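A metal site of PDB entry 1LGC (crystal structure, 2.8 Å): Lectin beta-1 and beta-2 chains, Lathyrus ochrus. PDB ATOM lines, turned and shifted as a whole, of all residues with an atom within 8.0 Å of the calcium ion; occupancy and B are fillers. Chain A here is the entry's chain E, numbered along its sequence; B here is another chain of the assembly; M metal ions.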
ATOM      1  N   VAL A  79      -6.324  25.345  12.317  1.00  0.00           N
ATOM      2  CA  VAL A  79      -6.794  24.383  13.309  1.00  0.00           C
ATOM      3  C   VAL A  79      -5.730  23.340  13.691  1.00  0.00           C
ATOM      4  O   VAL A  79      -4.983  22.862  12.840  1.00  0.00           O
ATOM      5  CB  VAL A  79      -8.053  23.615  12.817  1.00  0.00           C
ATOM      6  CG1 VAL A  79      -8.667  22.779  13.939  1.00  0.00           C
ATOM      7  CG2 VAL A  79      -9.075  24.584  12.258  1.00  0.00           C
ATOM      8  N   ALA A  80      -5.705  22.989  14.977  1.00  0.00           N
ATOM      9  CA  ALA A  80      -4.780  21.996  15.541  1.00  0.00           C
ATOM     10  C   ALA A  80      -5.279  21.609  16.946  1.00  0.00           C
ATOM     11  O   ALA A  80      -5.885  22.435  17.633  1.00  0.00           O
ATOM     12  CB  ALA A  80      -3.369  22.583  15.615  1.00  0.00           C
ATOM     13  N   ASP A  81      -5.044  20.373  17.386  1.00  0.00           N
ATOM     14  CA  ASP A  81      -4.333  19.384  16.599  1.00  0.00           C
ATOM     15  C   ASP A  81      -5.128  18.089  16.347  1.00  0.00           C
ATOM     16  O   ASP A  81      -4.762  17.313  15.466  1.00  0.00           O
ATOM     17  CB  ASP A  81      -3.003  19.051  17.286  1.00  0.00           C
ATOM     18  CG  ASP A  81      -2.027  18.422  16.339  1.00  0.00           C
ATOM     19  OD1 ASP A  81      -2.136  17.206  16.074  1.00  0.00           O
ATOM     20  OD2 ASP A  81      -1.160  19.158  15.814  1.00  0.00           O
ATOM     21  N   GLY A  82      -6.162  17.854  17.151  1.00  0.00           N
ATOM     22  CA  GLY A  82      -6.970  16.658  16.966  1.00  0.00           C
ATOM     23  C   GLY A  82      -7.642  16.115  18.223  1.00  0.00           C
ATOM     24  O   GLY A  82      -7.168  16.344  19.333  1.00  0.00           O
ATOM     25  N   GLY A  98       0.832  17.745  21.279  1.00  0.00           N
ATOM     26  CA  GLY A  98       0.967  18.092  19.883  1.00  0.00           C
ATOM     27  C   GLY A  98       0.286  17.107  18.968  1.00  0.00           C
ATOM     28  O   GLY A  98      -0.829  16.668  19.222  1.00  0.00           O
ATOM     29  N   GLY A  99       0.990  16.716  17.905  1.00  0.00           N
ATOM     30  CA  GLY A  99       0.446  15.780  16.945  1.00  0.00           C
ATOM     31  C   GLY A  99       0.150  14.416  17.520  1.00  0.00           C
ATOM     32  O   GLY A  99      -0.621  13.665  16.915  1.00  0.00           O
ATOM     33  N   TYR A 100       0.721  14.094  18.684  1.00  0.00           N
ATOM     34  CA  TYR A 100       0.512  12.788  19.301  1.00  0.00           C
ATOM     35  C   TYR A 100      -0.855  12.625  19.950  1.00  0.00           C
ATOM     36  O   TYR A 100      -1.161  11.569  20.519  1.00  0.00           O
ATOM     37  CB  TYR A 100       1.624  12.479  20.296  1.00  0.00           C
ATOM     38  CG  TYR A 100       2.961  12.322  19.640  1.00  0.00           C
ATOM     39  CD1 TYR A 100       3.791  13.422  19.429  1.00  0.00           C
ATOM     40  CD2 TYR A 100       3.401  11.078  19.190  1.00  0.00           C
ATOM     41  CE1 TYR A 100       5.011  13.289  18.793  1.00  0.00           C
ATOM     42  CE2 TYR A 100       4.609  10.939  18.536  1.00  0.00           C
ATOM     43  CZ  TYR A 100       5.420  12.048  18.347  1.00  0.00           C
ATOM     44  OH  TYR A 100       6.647  11.899  17.733  1.00  0.00           O
ATOM     45  N   LEU A 101      -1.656  13.692  19.889  1.00  0.00           N
ATOM     46  CA  LEU A 101      -3.004  13.687  20.430  1.00  0.00           C
ATOM     47  C   LEU A 101      -3.060  13.168  21.873  1.00  0.00           C
ATOM     48  O   LEU A 101      -4.029  12.526  22.284  1.00  0.00           O
ATOM     49  CB  LEU A 101      -3.931  12.868  19.518  1.00  0.00           C
ATOM     50  CG  LEU A 101      -3.966  13.200  18.012  1.00  0.00           C
ATOM     51  CD1 LEU A 101      -5.111  12.434  17.383  1.00  0.00           C
ATOM     52  CD2 LEU A 101      -4.188  14.693  17.775  1.00  0.00           C
ATOM     53  N   GLU A 119      -8.774   8.489  15.680  1.00  0.00           N
ATOM     54  CA  GLU A 119      -8.400   9.891  15.660  1.00  0.00           C
ATOM     55  C   GLU A 119      -9.038  10.792  14.607  1.00  0.00           C
ATOM     56  O   GLU A 119      -9.211  10.405  13.455  1.00  0.00           O
ATOM     57  CB  GLU A 119      -6.879  10.052  15.594  1.00  0.00           C
ATOM     58  CG  GLU A 119      -6.247   9.427  14.383  1.00  0.00           C
ATOM     59  CD  GLU A 119      -4.984  10.145  13.975  1.00  0.00           C
ATOM     60  OE1 GLU A 119      -3.908   9.847  14.555  1.00  0.00           O
ATOM     61  OE2 GLU A 119      -5.057  10.999  13.066  1.00  0.00           O
ATOM     62  N   PHE A 120      -9.350  12.002  15.026  1.00  0.00           N
ATOM     63  CA  PHE A 120      -9.937  13.003  14.175  1.00  0.00           C
ATOM     64  C   PHE A 120      -8.894  14.119  14.150  1.00  0.00           C
ATOM     65  O   PHE A 120      -9.077  15.179  14.771  1.00  0.00           O
ATOM     66  CB  PHE A 120     -11.262  13.481  14.790  1.00  0.00           C
ATOM     67  CG  PHE A 120     -12.271  12.375  14.983  1.00  0.00           C
ATOM     68  CD1 PHE A 120     -12.120  11.452  16.016  1.00  0.00           C
ATOM     69  CD2 PHE A 120     -13.326  12.202  14.097  1.00  0.00           C
ATOM     70  CE1 PHE A 120     -12.994  10.352  16.151  1.00  0.00           C
ATOM     71  CE2 PHE A 120     -14.196  11.123  14.218  1.00  0.00           C
ATOM     72  CZ  PHE A 120     -14.034  10.191  15.242  1.00  0.00           C
ATOM     73  N   ASP A 121      -7.761  13.844  13.476  1.00  0.00           N
ATOM     74  CA  ASP A 121      -6.650  14.790  13.367  1.00  0.00           C
ATOM     75  C   ASP A 121      -7.035  15.973  12.484  1.00  0.00           C
ATOM     76  O   ASP A 121      -7.622  15.803  11.409  1.00  0.00           O
ATOM     77  CB  ASP A 121      -5.388  14.083  12.796  1.00  0.00           C
ATOM     78  CG  ASP A 121      -4.077  14.896  12.969  1.00  0.00           C
ATOM     79  OD1 ASP A 121      -4.131  16.129  13.211  1.00  0.00           O
ATOM     80  OD2 ASP A 121      -2.970  14.312  12.856  1.00  0.00           O
ATOM     81  N   THR A 122      -6.656  17.177  12.933  1.00  0.00           N
ATOM     82  CA  THR A 122      -6.935  18.407  12.203  1.00  0.00           C
ATOM     83  C   THR A 122      -5.627  19.179  11.894  1.00  0.00           C
ATOM     84  O   THR A 122      -5.648  20.379  11.637  1.00  0.00           O
ATOM     85  CB  THR A 122      -7.909  19.289  13.008  1.00  0.00           C
ATOM     86  OG1 THR A 122      -7.274  19.738  14.217  1.00  0.00           O
ATOM     87  CG2 THR A 122      -9.153  18.497  13.363  1.00  0.00           C
ATOM     88  N   PHE A 123      -4.495  18.495  11.926  1.00  0.00           N
ATOM     89  CA  PHE A 123      -3.209  19.121  11.653  1.00  0.00           C
ATOM     90  C   PHE A 123      -2.329  18.105  10.972  1.00  0.00           C
ATOM     91  O   PHE A 123      -2.126  16.989  11.520  1.00  0.00           O
ATOM     92  CB  PHE A 123      -2.503  19.616  12.917  1.00  0.00           C
ATOM     93  CG  PHE A 123      -1.184  20.336  12.666  1.00  0.00           C
ATOM     94  CD1 PHE A 123      -1.156  21.711  12.458  1.00  0.00           C
ATOM     95  CD2 PHE A 123       0.029  19.662  12.697  1.00  0.00           C
ATOM     96  CE1 PHE A 123       0.045  22.411  12.285  1.00  0.00           C
ATOM     97  CE2 PHE A 123       1.242  20.355  12.524  1.00  0.00           C
ATOM     98  CZ  PHE A 123       1.240  21.733  12.329  1.00  0.00           C
ATOM     99  N   TYR A 124      -1.759  18.504   9.842  1.00  0.00           N
ATOM    100  CA  TYR A 124      -0.888  17.641   9.067  1.00  0.00           C
ATOM    101  C   TYR A 124       0.549  17.707   9.577  1.00  0.00           C
ATOM    102  O   TYR A 124       1.200  18.763   9.547  1.00  0.00           O
ATOM    103  CB  TYR A 124      -0.957  17.996   7.572  1.00  0.00           C
ATOM    104  CG  TYR A 124       0.118  17.362   6.716  1.00  0.00           C
ATOM    105  CD1 TYR A 124       0.247  15.973   6.653  1.00  0.00           C
ATOM    106  CD2 TYR A 124       1.026  18.148   6.005  1.00  0.00           C
ATOM    107  CE1 TYR A 124       1.266  15.392   5.918  1.00  0.00           C
ATOM    108  CE2 TYR A 124       2.031  17.584   5.269  1.00  0.00           C
ATOM    109  CZ  TYR A 124       2.160  16.208   5.224  1.00  0.00           C
ATOM    110  OH  TYR A 124       3.210  15.649   4.523  1.00  0.00           O
ATOM    111  N   ASN A 125       1.000  16.565  10.078  1.00  0.00           N
ATOM    112  CA  ASN A 125       2.334  16.380  10.619  1.00  0.00           C
ATOM    113  C   ASN A 125       3.082  15.586   9.563  1.00  0.00           C
ATOM    114  O   ASN A 125       2.902  14.370   9.439  1.00  0.00           O
ATOM    115  CB  ASN A 125       2.272  15.573  11.925  1.00  0.00           C
ATOM    116  CG  ASN A 125       1.362  16.211  12.975  1.00  0.00           C
ATOM    117  OD1 ASN A 125       0.173  15.859  13.081  1.00  0.00           O
ATOM    118  ND2 ASN A 125       1.905  17.153  13.740  1.00  0.00           N
ATOM    119  N   THR A 126       3.911  16.283   8.803  1.00  0.00           N
ATOM    120  CA  THR A 126       4.693  15.681   7.723  1.00  0.00           C
ATOM    121  C   THR A 126       5.354  14.333   8.059  1.00  0.00           C
ATOM    122  O   THR A 126       5.325  13.393   7.261  1.00  0.00           O
ATOM    123  CB  THR A 126       5.765  16.676   7.173  1.00  0.00           C
ATOM    124  OG1 THR A 126       6.758  16.932   8.186  1.00  0.00           O
ATOM    125  CG2 THR A 126       5.107  18.005   6.759  1.00  0.00           C
ATOM    126  N   TRP A 128       4.442  11.836   9.895  1.00  0.00           N
ATOM    127  CA  TRP A 128       3.616  10.639   9.988  1.00  0.00           C
ATOM    128  C   TRP A 128       2.195  10.750   9.448  1.00  0.00           C
ATOM    129  O   TRP A 128       1.416   9.793   9.539  1.00  0.00           O
ATOM    130  CB  TRP A 128       3.564  10.155  11.446  1.00  0.00           C
ATOM    131  CG  TRP A 128       2.965  11.159  12.380  1.00  0.00           C
ATOM    132  CD1 TRP A 128       1.649  11.510  12.463  1.00  0.00           C
ATOM    133  CD2 TRP A 128       3.651  11.974  13.332  1.00  0.00           C
ATOM    134  NE1 TRP A 128       1.473  12.488  13.402  1.00  0.00           N
ATOM    135  CE2 TRP A 128       2.681  12.802  13.951  1.00  0.00           C
ATOM    136  CE3 TRP A 128       4.995  12.096  13.732  1.00  0.00           C
ATOM    137  CZ2 TRP A 128       3.014  13.730  14.948  1.00  0.00           C
ATOM    138  CZ3 TRP A 128       5.317  13.020  14.721  1.00  0.00           C
ATOM    139  CH2 TRP A 128       4.329  13.821  15.316  1.00  0.00           C
ATOM    140  N   ASP A 129       1.836  11.896   8.874  1.00  0.00           N
ATOM    141  CA  ASP A 129       0.482  12.089   8.354  1.00  0.00           C
ATOM    142  C   ASP A 129       0.303  11.855   6.863  1.00  0.00           C
ATOM    143  O   ASP A 129       1.287  11.802   6.101  1.00  0.00           O
ATOM    144  CB  ASP A 129      -0.035  13.465   8.772  1.00  0.00           C
ATOM    145  CG  ASP A 129      -0.726  13.458  10.120  1.00  0.00           C
ATOM    146  OD1 ASP A 129      -1.303  12.414  10.506  1.00  0.00           O
ATOM    147  OD2 ASP A 129      -0.719  14.502  10.802  1.00  0.00           O
ATOM    148  N   PRO A 130      -0.960  11.664   6.413  1.00  0.00           N
ATOM    149  CA  PRO A 130      -1.274  11.437   4.999  1.00  0.00           C
ATOM    150  C   PRO A 130      -0.697  12.531   4.095  1.00  0.00           C
ATOM    151  O   PRO A 130      -0.805  13.726   4.400  1.00  0.00           O
ATOM    152  CB  PRO A 130      -2.803  11.442   4.998  1.00  0.00           C
ATOM    153  CG  PRO A 130      -3.114  10.744   6.276  1.00  0.00           C
ATOM    154  CD  PRO A 130      -2.159  11.442   7.245  1.00  0.00           C
ATOM    155  N   HIS A 136      -8.257  14.582   8.782  1.00  0.00           N
ATOM    156  CA  HIS A 136      -8.786  13.262   8.533  1.00  0.00           C
ATOM    157  C   HIS A 136      -9.046  12.404   9.758  1.00  0.00           C
ATOM    158  O   HIS A 136      -8.379  12.546  10.777  1.00  0.00           O
ATOM    159  CB  HIS A 136      -7.738  12.515   7.738  1.00  0.00           C
ATOM    160  CG  HIS A 136      -6.425  12.410   8.463  1.00  0.00           C
ATOM    161  ND1 HIS A 136      -5.451  13.387   8.387  1.00  0.00           N
ATOM    162  CD2 HIS A 136      -5.945  11.464   9.308  1.00  0.00           C
ATOM    163  CE1 HIS A 136      -4.438  13.047   9.164  1.00  0.00           C
ATOM    164  NE2 HIS A 136      -4.709  11.885   9.735  1.00  0.00           N
ATOM    165  N   ILE A 144       1.047   6.963  16.377  1.00  0.00           N
ATOM    166  CA  ILE A 144       0.302   8.135  15.967  1.00  0.00           C
ATOM    167  C   ILE A 144       0.170   8.159  14.440  1.00  0.00           C
ATOM    168  O   ILE A 144      -0.481   9.032  13.852  1.00  0.00           O
ATOM    169  CB  ILE A 144       1.013   9.405  16.437  1.00  0.00           C
ATOM    170  CG1 ILE A 144       0.063  10.594  16.406  1.00  0.00           C
ATOM    171  CG2 ILE A 144       2.273   9.645  15.626  1.00  0.00           C
ATOM    172  CD1 ILE A 144      -1.117  10.399  17.333  1.00  0.00           C
ATOM    173  N   THR B  27      -5.622  17.724  22.040  1.00  0.00           N
ATOM    174  CA  THR B  27      -4.373  18.390  22.325  1.00  0.00           C
ATOM    175  C   THR B  27      -4.192  19.528  21.340  1.00  0.00           C
ATOM    176  O   THR B  27      -4.944  19.640  20.363  1.00  0.00           O
ATOM    177  CB  THR B  27      -3.176  17.410  22.192  1.00  0.00           C
ATOM    178  OG1 THR B  27      -3.172  16.830  20.885  1.00  0.00           O
ATOM    179  CG2 THR B  27      -3.256  16.271  23.215  1.00  0.00           C
HETATM  180 CA    CA M   1      -1.684  16.411  13.463  1.00  0.00          CA
HETATM  181 MN    MN M   2      -3.157  11.687  12.036  1.00  0.00          MN
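OD2 of Asp 129 sits at hydrogen-bond distance from N of Asn 125 (2.8 Å).
N of His 136 lies within hydrogen-bond range of O of Asp 121, at 3.0 Å.
O of Asp 81 sits at hydrogen-bond distance from N of Thr 122 (3.2 Å).
The backbone carbonyl oxygen (O) of Thr 27 of chain B sits at hydrogen-bond distance from the backbone NH (N) of Asp 81 (3.1 Å).
Residues that only touch the calcium ion: Asp 129.
The nearest printed residue that does not touch the calcium ion is Gly 99 (4.1 Å).
The calcium ion is bound by the side-chain amide oxygen (OD1) of Asn 125, the backbone carbonyl oxygen (O) of Phe 123, the side-chain carboxylate (OD1) of Asp 121, the side-chain carboxylate (OD2) of Asp 121 and the side-chain carboxylate (OD1) of Asp 81.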
